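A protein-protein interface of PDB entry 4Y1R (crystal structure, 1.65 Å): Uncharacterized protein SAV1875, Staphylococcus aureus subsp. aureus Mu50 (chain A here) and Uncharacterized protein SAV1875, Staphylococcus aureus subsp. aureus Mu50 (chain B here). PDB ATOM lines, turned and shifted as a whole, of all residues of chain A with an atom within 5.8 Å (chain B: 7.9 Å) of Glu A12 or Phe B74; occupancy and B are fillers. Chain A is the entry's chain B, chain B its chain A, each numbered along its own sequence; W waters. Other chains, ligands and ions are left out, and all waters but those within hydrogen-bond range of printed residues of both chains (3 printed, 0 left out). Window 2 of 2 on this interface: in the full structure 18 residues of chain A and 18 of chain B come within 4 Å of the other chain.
Water W1 lies within hydrogen-bond range of the side-chain carboxylate of Asp B77 (2.8 Å), the side-chain amide nitrogen of Gln B109 (3.0 Å) and the side-chain carboxylate of Asp A77 (3.2 Å). Water W3 lies within hydrogen-bond range of the side-chain carboxylate of Asp A77 and the backbone carbonyl oxygen of Asn B127. Water W2 bridges the side-chain amide oxygen (OD1) of Asn B127 (3.1 Å) and a ring nitrogen (ND1) of His A78 (3.4 Å).
The backbone carbonyl oxygen (O) of Glu B12 lies within hydrogen-bond range of the backbone NH (N) of Ser B75 (3.4 Å). OD2 of OCS B105 is in hydrogen-bond range of a ring nitrogen (ND1) of His B106, 2.8 Å away. O of His B106 lies close to OE1 of Gln B109 (3.5 Å). The backbone carbonyl oxygen (O) of Val A44 sits at hydrogen-bond distance from the backbone NH (N) of Glu A12. The backbone carbonyl oxygen (O) of Glu A12 sits at hydrogen-bond distance from the backbone NH (N) of Phe A74, 2.8 Å away. OE1 of Glu A12 lies within hydrogen-bond range of NE2 of His A78 (2.5 Å).
Of the 22 printed residues of chain B, 6 touch a printed residue of chain A. Printed residues of chain A that touch a printed residue of chain B: Glu A12, Phe A74, Asp A77 and His A78. Hydrophobic or aromatic side chains of chain A within 4 Å of the printed part of chain B: Phe A74 and His A78. Among the printed residues, 9 pairs touch across the chains.
CE2 of Phe B74 touches OE1 of Glu A12, 3.4 Å away. CE2 of Phe A74 touches OE1 of Glu B12 (3.5 Å). CD2 of Phe A74 touches CD2 of Phe B74, at 3.5 Å. Asp B77 touches Phe A74. CZ of Phe A74 touches NE2 of His B78, at 3.9 Å. OD2 of Asp A77 touches CE1 of Phe B74, 3.5 Å away. CZ of Phe B74 touches CE1 of His A78 (3.8 Å).
OD1 of Asp A77 lies within hydrogen-bond range of NE2 of His B106 (2.8 Å). O of Asp A77 lies close to OD1 of Asn B127 (2.8 Å).
Of the printed residues of chain B, Asp A77 touches Phe B74, His B106 and Asn B127. Of the printed residues of chain B, His A78 touches Phe B74 (3.8 Å). Printed residues of chain A within 4 Å of Glu B12: Phe A74 (3.5 Å). Of the printed residues of chain A, Phe B74 touches Glu A12, Phe A74, Asp A77 and His A78. Of the printed residues of chain A, Asp B77 touches Phe A74. Printed residues of chain A within 4 Å of His B106: Asp A77 (2.8 Å). The nearest printed residue of chain A that does not touch Phe B74 is Ser A75 (6.4 Å). The nearest printed residue of chain A that does not touch Glu B12 is Glu A12 (4.4 Å).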
ATOM      1  N   ALA A  10       1.872  14.170  15.316  1.00  0.00           N
ATOM      2  CA  ALA A  10       1.069  15.391  15.204  1.00  0.00           C
ATOM      3  C   ALA A  10       1.717  16.322  14.187  1.00  0.00           C
ATOM      4  O   ALA A  10       2.742  15.988  13.589  1.00  0.00           O
ATOM      5  CB  ALA A  10       0.966  16.083  16.557  1.00  0.00           C
ATOM      6  N   ASN A  11       1.088  17.466  13.937  1.00  0.00           N
ATOM      7  CA  ASN A  11       1.674  18.448  13.020  1.00  0.00           C
ATOM      8  C   ASN A  11       3.043  18.919  13.510  1.00  0.00           C
ATOM      9  O   ASN A  11       3.308  18.924  14.710  1.00  0.00           O
ATOM     10  CB  ASN A  11       0.744  19.652  12.873  1.00  0.00           C
ATOM     11  CG  ASN A  11      -0.496  19.316  12.080  1.00  0.00           C
ATOM     12  OD1 ASN A  11      -0.414  18.989  10.903  1.00  0.00           O
ATOM     13  ND2 ASN A  11      -1.648  19.334  12.740  1.00  0.00           N
ATOM     14  N   GLU A  12       3.851  19.386  12.566  1.00  0.00           N
ATOM     15  CA  GLU A  12       5.160  19.979  12.834  1.00  0.00           C
ATOM     16  C   GLU A  12       6.161  18.986  13.383  1.00  0.00           C
ATOM     17  O   GLU A  12       7.099  19.365  14.086  1.00  0.00           O
ATOM     18  CB  GLU A  12       5.044  21.193  13.759  1.00  0.00           C
ATOM     19  CG  GLU A  12       4.042  22.206  13.241  1.00  0.00           C
ATOM     20  CD  GLU A  12       4.002  23.471  14.068  1.00  0.00           C
ATOM     21  OE1 GLU A  12       3.366  23.478  15.142  1.00  0.00           O
ATOM     22  OE2 GLU A  12       4.573  24.476  13.611  1.00  0.00           O
ATOM     23  N   PHE A  13       5.960  17.707  13.083  1.00  0.00           N
ATOM     24  CA  PHE A  13       7.052  16.754  13.208  1.00  0.00           C
ATOM     25  C   PHE A  13       8.211  17.153  12.310  1.00  0.00           C
ATOM     26  O   PHE A  13       8.017  17.818  11.276  1.00  0.00           O
ATOM     27  CB  PHE A  13       6.592  15.319  12.883  1.00  0.00           C
ATOM     28  CG  PHE A  13       6.115  15.139  11.458  1.00  0.00           C
ATOM     29  CD1 PHE A  13       4.794  15.384  11.139  1.00  0.00           C
ATOM     30  CD2 PHE A  13       6.962  14.633  10.475  1.00  0.00           C
ATOM     31  CE1 PHE A  13       4.347  15.276   9.824  1.00  0.00           C
ATOM     32  CE2 PHE A  13       6.500  14.439   9.184  1.00  0.00           C
ATOM     33  CZ  PHE A  13       5.188  14.724   8.867  1.00  0.00           C
ATOM     34  N   GLU A  14       9.427  16.826  12.746  1.00  0.00           N
ATOM     35  CA  GLU A  14      10.608  16.973  11.899  1.00  0.00           C
ATOM     36  C   GLU A  14      10.602  15.931  10.773  1.00  0.00           C
ATOM     37  O   GLU A  14      10.736  14.734  11.036  1.00  0.00           O
ATOM     38  CB  GLU A  14      11.884  16.810  12.736  1.00  0.00           C
ATOM     39  CG  GLU A  14      13.168  17.025  11.943  1.00  0.00           C
ATOM     40  CD  GLU A  14      13.356  18.466  11.503  1.00  0.00           C
ATOM     41  OE1 GLU A  14      13.310  19.370  12.356  1.00  0.00           O
ATOM     42  OE2 GLU A  14      13.617  18.699  10.314  1.00  0.00           O
ATOM     43  N   VAL A  44       1.165  17.591   8.932  1.00  0.00           N
ATOM     44  CA  VAL A  44       2.124  18.178   8.010  1.00  0.00           C
ATOM     45  C   VAL A  44       3.407  18.508   8.763  1.00  0.00           C
ATOM     46  O   VAL A  44       3.368  19.113   9.829  1.00  0.00           O
ATOM     47  CB  VAL A  44       1.553  19.459   7.352  1.00  0.00           C
ATOM     48  CG1 VAL A  44       2.584  20.074   6.423  1.00  0.00           C
ATOM     49  CG2 VAL A  44       0.282  19.122   6.587  1.00  0.00           C
ATOM     50  N   GLY A  45       4.544  18.113   8.204  1.00  0.00           N
ATOM     51  CA  GLY A  45       5.825  18.310   8.896  1.00  0.00           C
ATOM     52  C   GLY A  45       6.244  19.771   8.882  1.00  0.00           C
ATOM     53  O   GLY A  45       5.687  20.569   8.136  1.00  0.00           O
ATOM     54  N   LYS A  46       7.280  20.104   9.655  1.00  0.00           N
ATOM     55  CA  LYS A  46       7.889  21.452   9.597  1.00  0.00           C
ATOM     56  C   LYS A  46       8.299  21.877   8.201  1.00  0.00           C
ATOM     57  O   LYS A  46       8.349  23.081   7.915  1.00  0.00           O
ATOM     58  CB  LYS A  46       9.143  21.500  10.480  1.00  0.00           C
ATOM     59  CG  LYS A  46       8.883  21.251  11.948  1.00  0.00           C
ATOM     60  CD  LYS A  46      10.196  21.218  12.717  1.00  0.00           C
ATOM     61  CE  LYS A  46      10.488  22.563  13.356  1.00  0.00           C
ATOM     62  NZ  LYS A  46      11.230  22.383  14.633  1.00  0.00           N
ATOM     63  N   GLY A  72      10.567  13.532  16.294  1.00  0.00           N
ATOM     64  CA  GLY A  72      10.704  14.806  16.995  1.00  0.00           C
ATOM     65  C   GLY A  72      10.130  15.984  16.221  1.00  0.00           C
ATOM     66  O   GLY A  72       9.012  15.925  15.700  1.00  0.00           O
ATOM     67  N   GLY A  73      10.817  17.110  16.297  1.00  0.00           N
ATOM     68  CA  GLY A  73      10.176  18.375  15.941  1.00  0.00           C
ATOM     69  C   GLY A  73       9.239  18.792  17.057  1.00  0.00           C
ATOM     70  O   GLY A  73       9.506  18.522  18.216  1.00  0.00           O
ATOM     71  N   PHE A  74       8.182  19.519  16.702  1.00  0.00           N
ATOM     72  CA  PHE A  74       7.212  19.960  17.702  1.00  0.00           C
ATOM     73  C   PHE A  74       5.990  19.067  17.754  1.00  0.00           C
ATOM     74  O   PHE A  74       5.045  19.331  18.502  1.00  0.00           O
ATOM     75  CB  PHE A  74       6.814  21.424  17.446  1.00  0.00           C
ATOM     76  CG  PHE A  74       7.929  22.394  17.722  1.00  0.00           C
ATOM     77  CD1 PHE A  74       8.630  22.313  18.910  1.00  0.00           C
ATOM     78  CD2 PHE A  74       8.322  23.320  16.762  1.00  0.00           C
ATOM     79  CE1 PHE A  74       9.689  23.176  19.175  1.00  0.00           C
ATOM     80  CE2 PHE A  74       9.377  24.197  17.026  1.00  0.00           C
ATOM     81  CZ  PHE A  74      10.087  24.081  18.203  1.00  0.00           C
ATOM     82  N   SER A  75       6.064  17.938  17.058  1.00  0.00           N
ATOM     83  CA  SER A  75       4.999  16.943  17.133  1.00  0.00           C
ATOM     84  C   SER A  75       4.794  16.444  18.583  1.00  0.00           C
ATOM     85  O   SER A  75       3.658  16.425  19.057  1.00  0.00           O
ATOM     86  CB  SER A  75       5.303  15.794  16.169  1.00  0.00           C
ATOM     87  OG  SER A  75       4.437  14.691  16.398  1.00  0.00           O
ATOM     88  N   ASP A  77       5.442  17.886  21.425  1.00  0.00           N
ATOM     89  CA  ASP A  77       4.779  18.917  22.205  1.00  0.00           C
ATOM     90  C   ASP A  77       3.278  19.006  21.898  1.00  0.00           C
ATOM     91  O   ASP A  77       2.456  19.077  22.804  1.00  0.00           O
ATOM     92  CB  ASP A  77       5.452  20.272  21.983  1.00  0.00           C
ATOM     93  CG  ASP A  77       4.936  21.332  22.949  1.00  0.00           C
ATOM     94  OD1 ASP A  77       5.608  21.615  23.951  1.00  0.00           O
ATOM     95  OD2 ASP A  77       3.933  21.951  22.621  1.00  0.00           O
ATOM     96  N   HIS A  78       2.913  18.990  20.627  1.00  0.00           N
ATOM     97  CA  HIS A  78       1.477  18.958  20.281  1.00  0.00           C
ATOM     98  C   HIS A  78       0.761  17.778  20.910  1.00  0.00           C
ATOM     99  O   HIS A  78      -0.338  17.926  21.453  1.00  0.00           O
ATOM    100  CB  HIS A  78       1.289  18.953  18.779  1.00  0.00           C
ATOM    101  CG  HIS A  78       1.575  20.280  18.125  1.00  0.00           C
ATOM    102  ND1 HIS A  78       0.967  21.425  18.522  1.00  0.00           N
ATOM    103  CD2 HIS A  78       2.255  20.589  16.944  1.00  0.00           C
ATOM    104  CE1 HIS A  78       1.333  22.439  17.699  1.00  0.00           C
ATOM    105  NE2 HIS A  78       2.156  21.934  16.758  1.00  0.00           N
ATOM    106  N   ALA B  10      12.611  34.216  20.796  1.00  0.00           N
ATOM    107  CA  ALA B  10      13.148  33.496  19.653  1.00  0.00           C
ATOM    108  C   ALA B  10      12.066  33.381  18.576  1.00  0.00           C
ATOM    109  O   ALA B  10      10.928  33.807  18.767  1.00  0.00           O
ATOM    110  CB  ALA B  10      13.606  32.109  20.096  1.00  0.00           C
ATOM    111  N   ASN B  11      12.396  32.739  17.455  1.00  0.00           N
ATOM    112  CA  ASN B  11      11.380  32.453  16.445  1.00  0.00           C
ATOM    113  C   ASN B  11      10.248  31.593  16.984  1.00  0.00           C
ATOM    114  O   ASN B  11      10.421  30.821  17.940  1.00  0.00           O
ATOM    115  CB  ASN B  11      12.039  31.762  15.256  1.00  0.00           C
ATOM    116  CG  ASN B  11      12.923  32.705  14.469  1.00  0.00           C
ATOM    117  OD1 ASN B  11      12.434  33.677  13.907  1.00  0.00           O
ATOM    118  ND2 ASN B  11      14.251  32.512  14.560  1.00  0.00           N
ATOM    119  N   GLU B  12       9.098  31.728  16.341  1.00  0.00           N
ATOM    120  CA  GLU B  12       7.922  30.905  16.573  1.00  0.00           C
ATOM    121  C   GLU B  12       7.343  31.153  17.956  1.00  0.00           C
ATOM    122  O   GLU B  12       6.617  30.327  18.477  1.00  0.00           O
ATOM    123  CB  GLU B  12       8.224  29.421  16.356  1.00  0.00           C
ATOM    124  CG  GLU B  12       8.670  29.118  14.928  1.00  0.00           C
ATOM    125  CD  GLU B  12       8.891  27.636  14.700  1.00  0.00           C
ATOM    126  OE1 GLU B  12       9.929  27.105  15.151  1.00  0.00           O
ATOM    127  OE2 GLU B  12       8.104  27.040  13.954  1.00  0.00           O
ATOM    128  N   PHE B  13       7.521  32.357  18.472  1.00  0.00           N
ATOM    129  CA  PHE B  13       6.665  32.815  19.555  1.00  0.00           C
ATOM    130  C   PHE B  13       5.196  32.880  19.118  1.00  0.00           C
ATOM    131  O   PHE B  13       4.871  33.061  17.937  1.00  0.00           O
ATOM    132  CB  PHE B  13       7.134  34.187  20.068  1.00  0.00           C
ATOM    133  CG  PHE B  13       7.086  35.281  19.026  1.00  0.00           C
ATOM    134  CD1 PHE B  13       8.174  35.502  18.200  1.00  0.00           C
ATOM    135  CD2 PHE B  13       6.012  36.185  18.966  1.00  0.00           C
ATOM    136  CE1 PHE B  13       8.131  36.485  17.202  1.00  0.00           C
ATOM    137  CE2 PHE B  13       5.964  37.194  17.998  1.00  0.00           C
ATOM    138  CZ  PHE B  13       7.027  37.343  17.104  1.00  0.00           C
ATOM    139  N   GLU B  14       4.302  32.718  20.083  1.00  0.00           N
ATOM    140  CA  GLU B  14       2.893  32.914  19.807  1.00  0.00           C
ATOM    141  C   GLU B  14       2.634  34.424  19.720  1.00  0.00           C
ATOM    142  O   GLU B  14       2.759  35.131  20.720  1.00  0.00           O
ATOM    143  CB  GLU B  14       2.067  32.311  20.946  1.00  0.00           C
ATOM    144  CG  GLU B  14       0.564  32.454  20.763  1.00  0.00           C
ATOM    145  CD  GLU B  14       0.052  31.626  19.605  1.00  0.00           C
ATOM    146  OE1 GLU B  14       0.260  30.403  19.613  1.00  0.00           O
ATOM    147  OE2 GLU B  14      -0.707  32.162  18.790  1.00  0.00           O
ATOM    148  N   GLU B  17       0.905  36.657  22.290  1.00  0.00           N
ATOM    149  CA  GLU B  17       1.522  36.643  23.615  1.00  0.00           C
ATOM    150  C   GLU B  17       2.744  37.539  23.702  1.00  0.00           C
ATOM    151  O   GLU B  17       3.249  37.799  24.803  1.00  0.00           O
ATOM    152  CB  GLU B  17       1.900  35.212  23.994  1.00  0.00           C
ATOM    153  CG  GLU B  17       0.670  34.346  24.243  1.00  0.00           C
ATOM    154  CD  GLU B  17       0.982  32.889  24.468  1.00  0.00           C
ATOM    155  OE1 GLU B  17       2.165  32.502  24.601  1.00  0.00           O
ATOM    156  OE2 GLU B  17       0.003  32.106  24.439  1.00  0.00           O
ATOM    157  N   LYS B  46       4.762  32.486  15.166  1.00  0.00           N
ATOM    158  CA  LYS B  46       3.987  31.409  14.545  1.00  0.00           C
ATOM    159  C   LYS B  46       3.090  31.902  13.426  1.00  0.00           C
ATOM    160  O   LYS B  46       2.799  31.139  12.496  1.00  0.00           O
ATOM    161  CB  LYS B  46       3.161  30.676  15.611  1.00  0.00           C
ATOM    162  CG  LYS B  46       3.997  29.759  16.477  1.00  0.00           C
ATOM    163  CD  LYS B  46       3.195  29.176  17.631  1.00  0.00           C
ATOM    164  CE  LYS B  46       2.698  27.780  17.286  1.00  0.00           C
ATOM    165  NZ  LYS B  46       2.909  26.883  18.448  1.00  0.00           N
ATOM    166  N   PRO B  71       7.109  35.398  26.455  1.00  0.00           N
ATOM    167  CA  PRO B  71       5.996  34.926  25.617  1.00  0.00           C
ATOM    168  C   PRO B  71       6.129  33.446  25.290  1.00  0.00           C
ATOM    169  O   PRO B  71       7.235  32.904  25.346  1.00  0.00           O
ATOM    170  CB  PRO B  71       6.136  35.778  24.331  1.00  0.00           C
ATOM    171  CG  PRO B  71       6.845  37.024  24.815  1.00  0.00           C
ATOM    172  CD  PRO B  71       7.849  36.503  25.807  1.00  0.00           C
ATOM    173  N   GLY B  72       5.004  32.808  24.954  1.00  0.00           N
ATOM    174  CA  GLY B  72       4.973  31.367  24.721  1.00  0.00           C
ATOM    175  C   GLY B  72       5.025  31.071  23.231  1.00  0.00           C
ATOM    176  O   GLY B  72       5.868  31.604  22.508  1.00  0.00           O
ATOM    177  N   GLY B  73       4.285  30.047  22.825  1.00  0.00           N
ATOM    178  CA  GLY B  73       4.594  29.416  21.544  1.00  0.00           C
ATOM    179  C   GLY B  73       5.800  28.493  21.657  1.00  0.00           C
ATOM    180  O   GLY B  73       6.082  27.926  22.726  1.00  0.00           O
ATOM    181  N   PHE B  74       6.552  28.376  20.569  1.00  0.00           N
ATOM    182  CA  PHE B  74       7.737  27.526  20.562  1.00  0.00           C
ATOM    183  C   PHE B  74       9.008  28.354  20.758  1.00  0.00           C
ATOM    184  O   PHE B  74      10.119  27.800  20.780  1.00  0.00           O
ATOM    185  CB  PHE B  74       7.808  26.704  19.279  1.00  0.00           C
ATOM    186  CG  PHE B  74       6.703  25.686  19.165  1.00  0.00           C
ATOM    187  CD1 PHE B  74       6.378  24.896  20.258  1.00  0.00           C
ATOM    188  CD2 PHE B  74       5.966  25.566  18.009  1.00  0.00           C
ATOM    189  CE1 PHE B  74       5.354  23.967  20.182  1.00  0.00           C
ATOM    190  CE2 PHE B  74       4.982  24.592  17.906  1.00  0.00           C
ATOM    191  CZ  PHE B  74       4.627  23.858  19.023  1.00  0.00           C
ATOM    192  N   SER B  75       8.839  29.653  21.019  1.00  0.00           N
ATOM    193  CA  SER B  75       9.989  30.498  21.352  1.00  0.00           C
ATOM    194  C   SER B  75      10.760  30.017  22.596  1.00  0.00           C
ATOM    195  O   SER B  75      11.987  29.825  22.517  1.00  0.00           O
ATOM    196  CB  SER B  75       9.569  31.978  21.424  1.00  0.00           C
ATOM    197  OG  SER B  75      10.538  32.764  22.100  1.00  0.00           O
ATOM    198  N   PRO B  76      10.049  29.661  23.681  1.00  0.00           N
ATOM    199  CA  PRO B  76      10.855  29.193  24.832  1.00  0.00           C
ATOM    200  C   PRO B  76      11.666  27.908  24.586  1.00  0.00           C
ATOM    201  O   PRO B  76      12.842  27.828  24.961  1.00  0.00           O
ATOM    202  CB  PRO B  76       9.792  28.948  25.919  1.00  0.00           C
ATOM    203  CG  PRO B  76       8.717  29.936  25.604  1.00  0.00           C
ATOM    204  CD  PRO B  76       8.646  29.917  24.070  1.00  0.00           C
ATOM    205  N   ASP B  77      11.098  26.970  23.829  1.00  0.00           N
ATOM    206  CA  ASP B  77      11.845  25.765  23.449  1.00  0.00           C
ATOM    207  C   ASP B  77      13.090  26.122  22.633  1.00  0.00           C
ATOM    208  O   ASP B  77      14.188  25.655  22.934  1.00  0.00           O
ATOM    209  CB  ASP B  77      10.936  24.805  22.658  1.00  0.00           C
ATOM    210  CG  ASP B  77      11.600  23.457  22.408  1.00  0.00           C
ATOM    211  OD1 ASP B  77      11.257  22.499  23.123  1.00  0.00           O
ATOM    212  OD2 ASP B  77      12.459  23.358  21.510  1.00  0.00           O
ATOM    213  N   HIS B  78      12.969  27.068  21.703  1.00  0.00           N
ATOM    214  CA  HIS B  78      14.157  27.530  20.973  1.00  0.00           C
ATOM    215  C   HIS B  78      15.206  28.147  21.881  1.00  0.00           C
ATOM    216  O   HIS B  78      16.412  27.911  21.697  1.00  0.00           O
ATOM    217  CB  HIS B  78      13.785  28.518  19.870  1.00  0.00           C
ATOM    218  CG  HIS B  78      13.144  27.867  18.675  1.00  0.00           C
ATOM    219  ND1 HIS B  78      13.729  26.847  18.008  1.00  0.00           N
ATOM    220  CD2 HIS B  78      11.938  28.131  18.027  1.00  0.00           C
ATOM    221  CE1 HIS B  78      12.960  26.514  16.944  1.00  0.00           C
ATOM    222  NE2 HIS B  78      11.854  27.290  16.970  1.00  0.00           N
ATOM    223  N   LEU B  79      14.772  29.031  22.784  1.00  0.00           N
ATOM    224  CA  LEU B  79      15.710  29.664  23.725  1.00  0.00           C
ATOM    225  C   LEU B  79      16.454  28.601  24.542  1.00  0.00           C
ATOM    226  O   LEU B  79      17.640  28.759  24.859  1.00  0.00           O
ATOM    227  CB  LEU B  79      14.969  30.621  24.671  1.00  0.00           C
ATOM    228  CG  LEU B  79      14.317  31.788  23.925  1.00  0.00           C
ATOM    229  CD1 LEU B  79      13.399  32.559  24.860  1.00  0.00           C
ATOM    230  CD2 LEU B  79      15.385  32.713  23.328  1.00  0.00           C
ATOM    231  N   ARG B  80      15.761  27.525  24.874  1.00  0.00           N
ATOM    232  CA  ARG B  80      16.373  26.436  25.636  1.00  0.00           C
ATOM    233  C   ARG B  80      17.364  25.605  24.841  1.00  0.00           C
ATOM    234  O   ARG B  80      18.059  24.752  25.410  1.00  0.00           O
ATOM    235  CB  ARG B  80      15.287  25.547  26.266  1.00  0.00           C
ATOM    236  CG  ARG B  80      14.413  26.338  27.240  1.00  0.00           C
ATOM    237  CD  ARG B  80      13.348  25.457  27.864  1.00  0.00           C
ATOM    238  NE  ARG B  80      13.883  24.661  28.977  1.00  0.00           N
ATOM    239  CZ  ARG B  80      13.243  23.618  29.507  1.00  0.00           C
ATOM    240  NH1 ARG B  80      12.151  23.136  28.923  1.00  0.00           N
ATOM    241  NH2 ARG B  80      13.694  23.071  30.627  1.00  0.00           N
ATOM    242  N   OCS B 105       1.929  30.537  28.935  1.00  0.00           N
ATOM    243  CA  OCS B 105       1.786  29.367  28.017  1.00  0.00           C
ATOM    244  CB  OCS B 105       1.318  29.820  26.611  1.00  0.00           C
ATOM    245  SG  OCS B 105       1.122  28.776  25.285  1.00  0.00           S
ATOM    246  C   OCS B 105       2.989  28.456  28.134  1.00  0.00           C
ATOM    247  O   OCS B 105       3.188  27.863  29.173  1.00  0.00           O
ATOM    248  OD1 OCS B 105       0.768  27.177  25.376  1.00  0.00           O
ATOM    249  OD2 OCS B 105       2.418  28.723  24.608  1.00  0.00           O
ATOM    250  OD3 OCS B 105       0.252  29.492  24.375  1.00  0.00           O
ATOM    251  N   HIS B 106       3.874  28.419  27.129  1.00  0.00           N
ATOM    252  CA  HIS B 106       5.138  27.709  27.257  1.00  0.00           C
ATOM    253  C   HIS B 106       6.209  28.506  27.959  1.00  0.00           C
ATOM    254  O   HIS B 106       7.293  27.995  28.211  1.00  0.00           O
ATOM    255  CB  HIS B 106       5.677  27.289  25.880  1.00  0.00           C
ATOM    256  CG  HIS B 106       4.959  26.109  25.264  1.00  0.00           C
ATOM    257  ND1 HIS B 106       3.817  26.243  24.533  1.00  0.00           N
ATOM    258  CD2 HIS B 106       5.322  24.764  25.185  1.00  0.00           C
ATOM    259  CE1 HIS B 106       3.457  25.028  24.051  1.00  0.00           C
ATOM    260  NE2 HIS B 106       4.380  24.130  24.435  1.00  0.00           N
ATOM    261  N   GLY B 107       5.980  29.809  28.097  1.00  0.00           N
ATOM    262  CA  GLY B 107       6.961  30.704  28.736  1.00  0.00           C
ATOM    263  C   GLY B 107       7.614  30.142  29.998  1.00  0.00           C
ATOM    264  O   GLY B 107       8.835  30.186  30.151  1.00  0.00           O
ATOM    265  N   GLN B 109       8.593  27.346  30.688  1.00  0.00           N
ATOM    266  CA  GLN B 109       9.714  26.431  30.350  1.00  0.00           C
ATOM    267  C   GLN B 109      11.070  27.032  30.667  1.00  0.00           C
ATOM    268  O   GLN B 109      11.941  26.364  31.225  1.00  0.00           O
ATOM    269  CB  GLN B 109       9.658  26.028  28.878  1.00  0.00           C
ATOM    270  CG  GLN B 109       8.515  25.075  28.560  1.00  0.00           C
ATOM    271  CD  GLN B 109       8.572  24.622  27.117  1.00  0.00           C
ATOM    272  OE1 GLN B 109       8.551  25.441  26.195  1.00  0.00           O
ATOM    273  NE2 GLN B 109       8.713  23.299  26.906  1.00  0.00           N
ATOM    274  N   ASN B 127       0.628  21.480  28.083  1.00  0.00           N
ATOM    275  CA  ASN B 127       1.710  20.702  27.466  1.00  0.00           C
ATOM    276  C   ASN B 127       2.943  20.656  28.370  1.00  0.00           C
ATOM    277  O   ASN B 127       3.803  19.816  28.172  1.00  0.00           O
ATOM    278  CB  ASN B 127       2.167  21.308  26.122  1.00  0.00           C
ATOM    279  CG  ASN B 127       1.022  21.606  25.172  1.00  0.00           C
ATOM    280  OD1 ASN B 127       1.113  21.298  23.978  1.00  0.00           O
ATOM    281  ND2 ASN B 127      -0.071  22.171  25.684  1.00  0.00           N
HETATM  282  O   HOH W   1       8.751  21.925  24.197  1.00  0.00           O
HETATM  283  O   HOH W   2      -0.686  21.850  21.487  1.00  0.00           O
HETATM  284  O   HOH W   3       5.737  19.624  25.899  1.00  0.00           O
